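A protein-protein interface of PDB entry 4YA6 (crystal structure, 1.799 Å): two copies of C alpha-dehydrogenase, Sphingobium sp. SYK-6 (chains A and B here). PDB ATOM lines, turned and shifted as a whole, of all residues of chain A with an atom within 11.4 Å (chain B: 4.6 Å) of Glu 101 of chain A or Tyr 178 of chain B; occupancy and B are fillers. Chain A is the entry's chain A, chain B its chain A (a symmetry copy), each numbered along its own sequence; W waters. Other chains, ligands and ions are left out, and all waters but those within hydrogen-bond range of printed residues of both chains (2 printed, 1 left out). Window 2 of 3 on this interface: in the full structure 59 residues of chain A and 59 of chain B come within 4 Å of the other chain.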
ATOM      1  N   GLN A  96     -21.167  26.189 -13.820  1.00  0.00           N
ATOM      2  CA  GLN A  96     -20.394  27.336 -14.269  1.00  0.00           C
ATOM      3  C   GLN A  96     -18.930  26.932 -14.323  1.00  0.00           C
ATOM      4  O   GLN A  96     -18.326  26.605 -13.300  1.00  0.00           O
ATOM      5  CB  GLN A  96     -20.597  28.538 -13.346  1.00  0.00           C
ATOM      6  CG  GLN A  96     -20.085  29.846 -13.927  1.00  0.00           C
ATOM      7  CD  GLN A  96     -21.005  31.017 -13.633  1.00  0.00           C
ATOM      8  OE1 GLN A  96     -21.710  31.502 -14.517  1.00  0.00           O
ATOM      9  NE2 GLN A  96     -21.001  31.476 -12.389  1.00  0.00           N
ATOM     10  N   PHE A  97     -18.371  26.939 -15.528  1.00  0.00           N
ATOM     11  CA  PHE A  97     -17.022  26.440 -15.756  1.00  0.00           C
ATOM     12  C   PHE A  97     -15.993  27.562 -15.749  1.00  0.00           C
ATOM     13  O   PHE A  97     -16.309  28.718 -16.034  1.00  0.00           O
ATOM     14  CB  PHE A  97     -16.966  25.686 -17.086  1.00  0.00           C
ATOM     15  CG  PHE A  97     -17.917  24.524 -17.165  1.00  0.00           C
ATOM     16  CD1 PHE A  97     -18.180  23.748 -16.047  1.00  0.00           C
ATOM     17  CD2 PHE A  97     -18.552  24.212 -18.354  1.00  0.00           C
ATOM     18  CE1 PHE A  97     -19.053  22.681 -16.117  1.00  0.00           C
ATOM     19  CE2 PHE A  97     -19.427  23.144 -18.428  1.00  0.00           C
ATOM     20  CZ  PHE A  97     -19.678  22.380 -17.308  1.00  0.00           C
ATOM     21  N   GLY A  98     -14.757  27.206 -15.417  1.00  0.00           N
ATOM     22  CA  GLY A  98     -13.659  28.151 -15.403  1.00  0.00           C
ATOM     23  C   GLY A  98     -12.453  27.539 -14.721  1.00  0.00           C
ATOM     24  O   GLY A  98     -12.586  26.524 -14.038  1.00  0.00           O
ATOM     25  N   PRO A  99     -11.269  28.145 -14.903  1.00  0.00           N
ATOM     26  CA  PRO A  99     -10.056  27.648 -14.245  1.00  0.00           C
ATOM     27  C   PRO A  99     -10.248  27.577 -12.738  1.00  0.00           C
ATOM     28  O   PRO A  99     -10.779  28.516 -12.148  1.00  0.00           O
ATOM     29  CB  PRO A  99      -8.994  28.685 -14.618  1.00  0.00           C
ATOM     30  CG  PRO A  99      -9.512  29.337 -15.851  1.00  0.00           C
ATOM     31  CD  PRO A  99     -11.001  29.347 -15.712  1.00  0.00           C
ATOM     32  N   ILE A 100      -9.824  26.479 -12.125  1.00  0.00           N
ATOM     33  CA  ILE A 100     -10.128  26.255 -10.720  1.00  0.00           C
ATOM     34  C   ILE A 100      -9.449  27.302  -9.838  1.00  0.00           C
ATOM     35  O   ILE A 100      -9.983  27.681  -8.798  1.00  0.00           O
ATOM     36  CB  ILE A 100      -9.715  24.833 -10.269  1.00  0.00           C
ATOM     37  CG1 ILE A 100     -10.235  24.539  -8.857  1.00  0.00           C
ATOM     38  CG2 ILE A 100      -8.202  24.655 -10.326  1.00  0.00           C
ATOM     39  CD1 ILE A 100     -11.743  24.624  -8.712  1.00  0.00           C
ATOM     40  N   GLU A 101      -8.292  27.796 -10.268  1.00  0.00           N
ATOM     41  CA  GLU A 101      -7.549  28.765  -9.467  1.00  0.00           C
ATOM     42  C   GLU A 101      -8.238  30.131  -9.446  1.00  0.00           C
ATOM     43  O   GLU A 101      -7.884  30.993  -8.642  1.00  0.00           O
ATOM     44  CB  GLU A 101      -6.110  28.912  -9.981  1.00  0.00           C
ATOM     45  CG  GLU A 101      -5.957  29.584 -11.346  1.00  0.00           C
ATOM     46  CD  GLU A 101      -6.052  28.613 -12.509  1.00  0.00           C
ATOM     47  OE1 GLU A 101      -6.513  27.471 -12.307  1.00  0.00           O
ATOM     48  OE2 GLU A 101      -5.658  28.997 -13.631  1.00  0.00           O
ATOM     49  N   LYS A 102      -9.217  30.319 -10.329  1.00  0.00           N
ATOM     50  CA  LYS A 102      -9.958  31.577 -10.414  1.00  0.00           C
ATOM     51  C   LYS A 102     -11.325  31.483  -9.735  1.00  0.00           C
ATOM     52  O   LYS A 102     -12.036  32.477  -9.623  1.00  0.00           O
ATOM     53  CB  LYS A 102     -10.142  31.992 -11.876  1.00  0.00           C
ATOM     54  CG  LYS A 102      -8.840  32.182 -12.650  1.00  0.00           C
ATOM     55  CD  LYS A 102      -7.980  33.309 -12.086  1.00  0.00           C
ATOM     56  CE  LYS A 102      -8.633  34.672 -12.267  1.00  0.00           C
ATOM     57  NZ  LYS A 102      -7.756  35.775 -11.789  1.00  0.00           N
ATOM     58  N   ALA A 103     -11.690  30.286  -9.288  1.00  0.00           N
ATOM     59  CA  ALA A 103     -12.980  30.074  -8.640  1.00  0.00           C
ATOM     60  C   ALA A 103     -13.073  30.831  -7.319  1.00  0.00           C
ATOM     61  O   ALA A 103     -12.103  30.907  -6.567  1.00  0.00           O
ATOM     62  CB  ALA A 103     -13.211  28.592  -8.408  1.00  0.00           C
ATOM     63  N   THR A 104     -14.250  31.389  -7.045  1.00  0.00           N
ATOM     64  CA  THR A 104     -14.509  32.072  -5.782  1.00  0.00           C
ATOM     65  C   THR A 104     -15.229  31.127  -4.828  1.00  0.00           C
ATOM     66  O   THR A 104     -15.761  30.101  -5.248  1.00  0.00           O
ATOM     67  CB  THR A 104     -15.369  33.339  -5.977  1.00  0.00           C
ATOM     68  OG1 THR A 104     -16.687  32.967  -6.400  1.00  0.00           O
ATOM     69  CG2 THR A 104     -14.743  34.267  -7.013  1.00  0.00           C
ATOM     70  N   PHE A 105     -15.251  31.467  -3.544  1.00  0.00           N
ATOM     71  CA  PHE A 105     -16.012  30.679  -2.583  1.00  0.00           C
ATOM     72  C   PHE A 105     -17.503  30.737  -2.916  1.00  0.00           C
ATOM     73  O   PHE A 105     -18.230  29.765  -2.706  1.00  0.00           O
ATOM     74  CB  PHE A 105     -15.756  31.170  -1.155  1.00  0.00           C
ATOM     75  CG  PHE A 105     -14.470  30.665  -0.560  1.00  0.00           C
ATOM     76  CD1 PHE A 105     -14.172  29.312  -0.559  1.00  0.00           C
ATOM     77  CD2 PHE A 105     -13.553  31.546  -0.007  1.00  0.00           C
ATOM     78  CE1 PHE A 105     -12.993  28.847  -0.014  1.00  0.00           C
ATOM     79  CE2 PHE A 105     -12.370  31.083   0.538  1.00  0.00           C
ATOM     80  CZ  PHE A 105     -12.092  29.733   0.533  1.00  0.00           C
ATOM     81  N   ASP A 106     -17.958  31.867  -3.451  1.00  0.00           N
ATOM     82  CA  ASP A 106     -19.353  31.997  -3.860  1.00  0.00           C
ATOM     83  C   ASP A 106     -19.675  31.047  -5.012  1.00  0.00           C
ATOM     84  O   ASP A 106     -20.775  30.493  -5.075  1.00  0.00           O
ATOM     85  CB  ASP A 106     -19.674  33.439  -4.269  1.00  0.00           C
ATOM     86  CG  ASP A 106     -19.764  34.381  -3.081  1.00  0.00           C
ATOM     87  OD1 ASP A 106     -19.895  33.897  -1.938  1.00  0.00           O
ATOM     88  OD2 ASP A 106     -19.713  35.611  -3.293  1.00  0.00           O
ATOM     89  N   ASP A 107     -18.718  30.869  -5.921  1.00  0.00           N
ATOM     90  CA  ASP A 107     -18.864  29.916  -7.020  1.00  0.00           C
ATOM     91  C   ASP A 107     -19.037  28.508  -6.468  1.00  0.00           C
ATOM     92  O   ASP A 107     -19.921  27.764  -6.897  1.00  0.00           O
ATOM     93  CB  ASP A 107     -17.652  29.957  -7.957  1.00  0.00           C
ATOM     94  CG  ASP A 107     -17.554  31.252  -8.744  1.00  0.00           C
ATOM     95  OD1 ASP A 107     -18.595  31.907  -8.957  1.00  0.00           O
ATOM     96  OD2 ASP A 107     -16.429  31.606  -9.157  1.00  0.00           O
ATOM     97  N   TRP A 108     -18.183  28.150  -5.513  1.00  0.00           N
ATOM     98  CA  TRP A 108     -18.255  26.842  -4.868  1.00  0.00           C
ATOM     99  C   TRP A 108     -19.590  26.633  -4.161  1.00  0.00           C
ATOM    100  O   TRP A 108     -20.280  25.641  -4.401  1.00  0.00           O
ATOM    101  CB  TRP A 108     -17.117  26.676  -3.857  1.00  0.00           C
ATOM    102  CG  TRP A 108     -15.835  26.140  -4.437  1.00  0.00           C
ATOM    103  CD1 TRP A 108     -14.688  26.838  -4.679  1.00  0.00           C
ATOM    104  CD2 TRP A 108     -15.572  24.787  -4.831  1.00  0.00           C
ATOM    105  NE1 TRP A 108     -13.726  26.003  -5.202  1.00  0.00           N
ATOM    106  CE2 TRP A 108     -14.246  24.741  -5.308  1.00  0.00           C
ATOM    107  CE3 TRP A 108     -16.330  23.613  -4.832  1.00  0.00           C
ATOM    108  CZ2 TRP A 108     -13.663  23.566  -5.778  1.00  0.00           C
ATOM    109  CZ3 TRP A 108     -15.745  22.447  -5.302  1.00  0.00           C
ATOM    110  CH2 TRP A 108     -14.427  22.433  -5.766  1.00  0.00           C
ATOM    111  N   LEU A 151     -12.375  17.184 -16.230  1.00  0.00           N
ATOM    112  CA  LEU A 151     -12.033  17.920 -17.443  1.00  0.00           C
ATOM    113  C   LEU A 151     -11.540  19.317 -17.084  1.00  0.00           C
ATOM    114  O   LEU A 151     -11.885  19.844 -16.026  1.00  0.00           O
ATOM    115  CB  LEU A 151     -13.252  18.018 -18.368  1.00  0.00           C
ATOM    116  CG  LEU A 151     -13.338  17.271 -19.707  1.00  0.00           C
ATOM    117  CD1 LEU A 151     -12.413  16.066 -19.813  1.00  0.00           C
ATOM    118  CD2 LEU A 151     -14.783  16.834 -19.930  1.00  0.00           C
ATOM    119  N   PRO A 152     -10.728  19.927 -17.963  1.00  0.00           N
ATOM    120  CA  PRO A 152     -10.329  21.320 -17.742  1.00  0.00           C
ATOM    121  C   PRO A 152     -11.535  22.245 -17.564  1.00  0.00           C
ATOM    122  O   PRO A 152     -12.477  22.174 -18.348  1.00  0.00           O
ATOM    123  CB  PRO A 152      -9.552  21.669 -19.016  1.00  0.00           C
ATOM    124  CG  PRO A 152      -9.040  20.369 -19.513  1.00  0.00           C
ATOM    125  CD  PRO A 152     -10.081  19.350 -19.155  1.00  0.00           C
ATOM    126  N   THR A 153     -11.489  23.076 -16.524  1.00  0.00           N
ATOM    127  CA  THR A 153     -12.508  24.089 -16.215  1.00  0.00           C
ATOM    128  C   THR A 153     -13.800  23.548 -15.586  1.00  0.00           C
ATOM    129  O   THR A 153     -14.703  24.333 -15.295  1.00  0.00           O
ATOM    130  CB  THR A 153     -12.920  24.916 -17.470  1.00  0.00           C
ATOM    131  OG1 THR A 153     -13.795  24.150 -18.312  1.00  0.00           O
ATOM    132  CG2 THR A 153     -11.694  25.390 -18.254  1.00  0.00           C
ATOM    133  N   THR A 154     -13.895  22.239 -15.358  1.00  0.00           N
ATOM    134  CA  THR A 154     -15.108  21.660 -14.763  1.00  0.00           C
ATOM    135  C   THR A 154     -14.897  21.202 -13.320  1.00  0.00           C
ATOM    136  O   THR A 154     -15.628  20.344 -12.828  1.00  0.00           O
ATOM    137  CB  THR A 154     -15.627  20.449 -15.573  1.00  0.00           C
ATOM    138  OG1 THR A 154     -14.753  19.325 -15.395  1.00  0.00           O
ATOM    139  CG2 THR A 154     -15.739  20.791 -17.052  1.00  0.00           C
ATOM    140  N   GLY A 155     -13.912  21.790 -12.647  1.00  0.00           N
ATOM    141  CA  GLY A 155     -13.522  21.366 -11.310  1.00  0.00           C
ATOM    142  C   GLY A 155     -14.636  21.348 -10.278  1.00  0.00           C
ATOM    143  O   GLY A 155     -14.845  20.338  -9.599  1.00  0.00           O
ATOM    144  N   ILE A 156     -15.349  22.461 -10.141  1.00  0.00           N
ATOM    145  CA  ILE A 156     -16.442  22.538  -9.175  1.00  0.00           C
ATOM    146  C   ILE A 156     -17.553  21.569  -9.561  1.00  0.00           C
ATOM    147  O   ILE A 156     -18.008  20.771  -8.741  1.00  0.00           O
ATOM    148  CB  ILE A 156     -17.015  23.969  -9.071  1.00  0.00           C
ATOM    149  CG1 ILE A 156     -15.929  24.934  -8.586  1.00  0.00           C
ATOM    150  CG2 ILE A 156     -18.211  23.999  -8.122  1.00  0.00           C
ATOM    151  CD1 ILE A 156     -16.356  26.391  -8.539  1.00  0.00           C
ATOM    152  N   THR A 159     -16.744  18.001  -8.940  1.00  0.00           N
ATOM    153  CA  THR A 159     -16.793  17.695  -7.514  1.00  0.00           C
ATOM    154  C   THR A 159     -18.234  17.425  -7.069  1.00  0.00           C
ATOM    155  O   THR A 159     -18.483  16.480  -6.320  1.00  0.00           O
ATOM    156  CB  THR A 159     -16.186  18.841  -6.668  1.00  0.00           C
ATOM    157  OG1 THR A 159     -14.841  19.089  -7.094  1.00  0.00           O
ATOM    158  CG2 THR A 159     -16.165  18.480  -5.192  1.00  0.00           C
ATOM    159  N   MET B 127      -3.556  27.032  -2.931  1.00  0.00           N
ATOM    160  CA  MET B 127      -3.199  26.754  -4.320  1.00  0.00           C
ATOM    161  C   MET B 127      -2.999  28.034  -5.144  1.00  0.00           C
ATOM    162  O   MET B 127      -2.062  28.111  -5.942  1.00  0.00           O
ATOM    163  CB  MET B 127      -4.265  25.853  -4.953  1.00  0.00           C
ATOM    164  CG  MET B 127      -4.132  25.634  -6.444  1.00  0.00           C
ATOM    165  SD  MET B 127      -5.293  26.655  -7.362  1.00  0.00           S
ATOM    166  CE  MET B 127      -6.877  25.999  -6.826  1.00  0.00           C
ATOM    167  N   PRO B 128      -3.862  29.047  -4.955  1.00  0.00           N
ATOM    168  CA  PRO B 128      -3.598  30.304  -5.668  1.00  0.00           C
ATOM    169  C   PRO B 128      -2.287  30.968  -5.245  1.00  0.00           C
ATOM    170  O   PRO B 128      -1.678  31.672  -6.052  1.00  0.00           O
ATOM    171  CB  PRO B 128      -4.799  31.180  -5.293  1.00  0.00           C
ATOM    172  CG  PRO B 128      -5.880  30.214  -4.960  1.00  0.00           C
ATOM    173  CD  PRO B 128      -5.183  29.060  -4.298  1.00  0.00           C
ATOM    174  N   ILE B 131       0.521  29.112  -7.153  1.00  0.00           N
ATOM    175  CA  ILE B 131       0.557  29.536  -8.547  1.00  0.00           C
ATOM    176  C   ILE B 131       1.189  30.921  -8.669  1.00  0.00           C
ATOM    177  O   ILE B 131       2.018  31.157  -9.547  1.00  0.00           O
ATOM    178  CB  ILE B 131      -0.862  29.542  -9.159  1.00  0.00           C
ATOM    179  CG1 ILE B 131      -1.374  28.105  -9.290  1.00  0.00           C
ATOM    180  CG2 ILE B 131      -0.869  30.226 -10.528  1.00  0.00           C
ATOM    181  CD1 ILE B 131      -2.832  27.992  -9.693  1.00  0.00           C
ATOM    182  N   GLY B 136       6.037  26.099  -8.127  1.00  0.00           N
ATOM    183  CA  GLY B 136       5.385  24.807  -8.059  1.00  0.00           C
ATOM    184  C   GLY B 136       4.978  24.471  -6.639  1.00  0.00           C
ATOM    185  O   GLY B 136       4.917  25.345  -5.775  1.00  0.00           O
ATOM    186  N   GLU B 174      -5.584  20.257 -13.959  1.00  0.00           N
ATOM    187  CA  GLU B 174      -5.268  21.674 -14.131  1.00  0.00           C
ATOM    188  C   GLU B 174      -3.975  22.125 -13.451  1.00  0.00           C
ATOM    189  O   GLU B 174      -3.436  23.177 -13.785  1.00  0.00           O
ATOM    190  CB  GLU B 174      -6.433  22.524 -13.615  1.00  0.00           C
ATOM    191  CG  GLU B 174      -7.753  22.242 -14.328  1.00  0.00           C
ATOM    192  CD  GLU B 174      -8.849  23.239 -13.986  1.00  0.00           C
ATOM    193  OE1 GLU B 174      -8.531  24.413 -13.699  1.00  0.00           O
ATOM    194  OE2 GLU B 174     -10.034  22.848 -14.012  1.00  0.00           O
ATOM    195  N   MET B 175      -3.471  21.339 -12.505  1.00  0.00           N
ATOM    196  CA  MET B 175      -2.299  21.749 -11.730  1.00  0.00           C
ATOM    197  C   MET B 175      -0.936  21.501 -12.399  1.00  0.00           C
ATOM    198  O   MET B 175       0.001  22.266 -12.162  1.00  0.00           O
ATOM    199  CB  MET B 175      -2.312  21.054 -10.366  1.00  0.00           C
ATOM    200  CG  MET B 175      -3.373  21.580  -9.403  1.00  0.00           C
ATOM    201  SD  MET B 175      -3.269  23.361  -9.118  1.00  0.00           S
ATOM    202  CE  MET B 175      -4.529  23.964 -10.243  1.00  0.00           C
ATOM    203  N   PRO B 176      -0.804  20.439 -13.216  1.00  0.00           N
ATOM    204  CA  PRO B 176       0.517  20.160 -13.796  1.00  0.00           C
ATOM    205  C   PRO B 176       1.136  21.317 -14.584  1.00  0.00           C
ATOM    206  O   PRO B 176       2.361  21.445 -14.589  1.00  0.00           O
ATOM    207  CB  PRO B 176       0.243  18.973 -14.720  1.00  0.00           C
ATOM    208  CG  PRO B 176      -0.894  18.270 -14.081  1.00  0.00           C
ATOM    209  CD  PRO B 176      -1.758  19.351 -13.496  1.00  0.00           C
ATOM    210  N   LYS B 177       0.321  22.146 -15.228  1.00  0.00           N
ATOM    211  CA  LYS B 177       0.857  23.256 -16.013  1.00  0.00           C
ATOM    212  C   LYS B 177       1.489  24.316 -15.112  1.00  0.00           C
ATOM    213  O   LYS B 177       2.231  25.177 -15.588  1.00  0.00           O
ATOM    214  CB  LYS B 177      -0.234  23.881 -16.888  1.00  0.00           C
ATOM    215  CG  LYS B 177      -1.390  24.516 -16.138  1.00  0.00           C
ATOM    216  CD  LYS B 177      -2.363  25.164 -17.117  1.00  0.00           C
ATOM    217  CE  LYS B 177      -3.546  25.810 -16.411  1.00  0.00           C
ATOM    218  NZ  LYS B 177      -4.378  24.822 -15.672  1.00  0.00           N
ATOM    219  N   TYR B 178       1.198  24.242 -13.816  1.00  0.00           N
ATOM    220  CA  TYR B 178       1.799  25.132 -12.828  1.00  0.00           C
ATOM    221  C   TYR B 178       2.883  24.423 -12.021  1.00  0.00           C
ATOM    222  O   TYR B 178       3.334  24.936 -10.998  1.00  0.00           O
ATOM    223  CB  TYR B 178       0.735  25.682 -11.874  1.00  0.00           C
ATOM    224  CG  TYR B 178      -0.320  26.528 -12.545  1.00  0.00           C
ATOM    225  CD1 TYR B 178       0.016  27.717 -13.179  1.00  0.00           C
ATOM    226  CD2 TYR B 178      -1.655  26.149 -12.530  1.00  0.00           C
ATOM    227  CE1 TYR B 178      -0.945  28.496 -13.788  1.00  0.00           C
ATOM    228  CE2 TYR B 178      -2.623  26.923 -13.135  1.00  0.00           C
ATOM    229  CZ  TYR B 178      -2.263  28.096 -13.763  1.00  0.00           C
ATOM    230  OH  TYR B 178      -3.224  28.870 -14.370  1.00  0.00           O
ATOM    231  N   ASN B 179       3.292  23.243 -12.487  1.00  0.00           N
ATOM    232  CA  ASN B 179       4.279  22.422 -11.788  1.00  0.00           C
ATOM    233  C   ASN B 179       3.849  22.110 -10.352  1.00  0.00           C
ATOM    234  O   ASN B 179       4.679  22.026  -9.444  1.00  0.00           O
ATOM    235  CB  ASN B 179       5.649  23.107 -11.791  1.00  0.00           C
ATOM    236  CG  ASN B 179       6.239  23.221 -13.184  1.00  0.00           C
ATOM    237  OD1 ASN B 179       6.091  22.319 -14.010  1.00  0.00           O
ATOM    238  ND2 ASN B 179       6.911  24.334 -13.452  1.00  0.00           N
ATOM    239  N   ILE B 180       2.543  21.942 -10.163  1.00  0.00           N
ATOM    240  CA  ILE B 180       1.989  21.565  -8.868  1.00  0.00           C
ATOM    241  C   ILE B 180       1.490  20.127  -8.932  1.00  0.00           C
ATOM    242  O   ILE B 180       0.579  19.809  -9.697  1.00  0.00           O
ATOM    243  CB  ILE B 180       0.842  22.511  -8.445  1.00  0.00           C
ATOM    244  CG1 ILE B 180       1.387  23.925  -8.233  1.00  0.00           C
ATOM    245  CG2 ILE B 180       0.171  22.013  -7.165  1.00  0.00           C
ATOM    246  CD1 ILE B 180       0.319  24.993  -8.114  1.00  0.00           C
HETATM  247  O   HOH W   1      -6.460  26.090 -14.379  1.00  0.00           O
HETATM  248  O   HOH W   2     -10.510  20.173 -13.410  1.00  0.00           O
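No position is printed for both chains.
Among the printed residues, pairs that only touch across the chains: Glu 101 of chain A with Ile 131 of chain B, Glu 101 of chain A with Met 127 of chain B, Pro 99 of chain A with Glu 174 of chain B, Ile 100 of chain A with Met 175 of chain B, Pro 152 of chain A with Glu 174 of chain B, Glu 101 of chain A with Glu 174 of chain B and Ile 100 of chain A with Met 127 of chain B.
Printed residues of chain B that touch a printed residue of chain A: Met 127, Ile 131, Glu 174, Met 175 and Tyr 178. Of the 20 printed residues of chain A, 5 touch a printed residue of chain B. Hydrophobic or aromatic side chains of chain A that line the printed part of chain B: Ile 100.
Water W1 lies within hydrogen-bond range of OE1 of Glu 101 of chain A (2.5 Å), OE1 of Glu 174 of chain B (2.8 Å) and NZ of Lys 177 of chain B (2.8 Å). Water W2 bridges the side-chain carboxylate of Glu 174 of chain B (2.8 Å) and the backbone carbonyl oxygen of Leu 151 of chain A (3.0 Å).
N of Gly 98 of chain A lies within hydrogen-bond range of O of Thr 153 of chain A, 2.9 Å away. The side-chain amino group of Lys 177 of chain B lies within hydrogen-bond range of the backbone carbonyl oxygen of Glu 174 of chain B (2.7 Å). O of Met 175 of chain B sits at hydrogen-bond distance from N of Ile 180 of chain B, 3.3 Å away.
Glu 101 of chain A touches just these residues of chain B: Met 127 (3.6 Å), Ile 131 (3.4 Å), Glu 174 (3.9 Å) and Tyr 178 (2.5 Å). No residue of chain A comes within 4 Å of Pro 128 of chain B. No residue of chain A comes within 4 Å of Gly 136 of chain B. Of chain A, only Pro 99, Ile 100, Glu 101, Pro 152 and Thr 153 come within 4 Å of Glu 174 of chain B. Met 175 of chain B touches just one residue of chain A: Ile 100 (3.7 Å). No residue of chain A comes within 4 Å of Pro 176 of chain B. No residue of chain A comes within 4 Å of Lys 177 of chain B. No residue of chain A comes within 4 Å of Ile 180 of chain B. Of the printed residues of chain B, Pro 152 of chain A touches Glu 174 (3.9 Å). Printed residues of chain B within 4 Å of Ile 100 of chain A: Met 127 (3.98 Å), Glu 174 (2.9 Å) and Met 175 (3.7 Å). Of the printed residues of chain B, Thr 153 of chain A touches Glu 174. Of the printed residues of chain A, Met 127 of chain B touches Ile 100 (3.98 Å) and Glu 101 (3.6 Å). Printed residues of chain B within 4 Å of Pro 99 of chain A: Glu 174. Lys 102 of chain A touches none of the printed residues of chain B. Thr 154 of chain A touches none of the printed residues of chain B.
The side-chain carboxylate of Glu 174 of chain B sits at hydrogen-bond distance from the backbone NH of Ile 100 of chain A, at 2.9 Å. OE2 of Glu 101 of chain A is in hydrogen-bond range of OH of Tyr 178 of chain B, 2.5 Å away. The backbone NH of Thr 153 of chain A is in hydrogen-bond range of the side-chain carboxylate of Glu 174 of chain B (2.9 Å).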
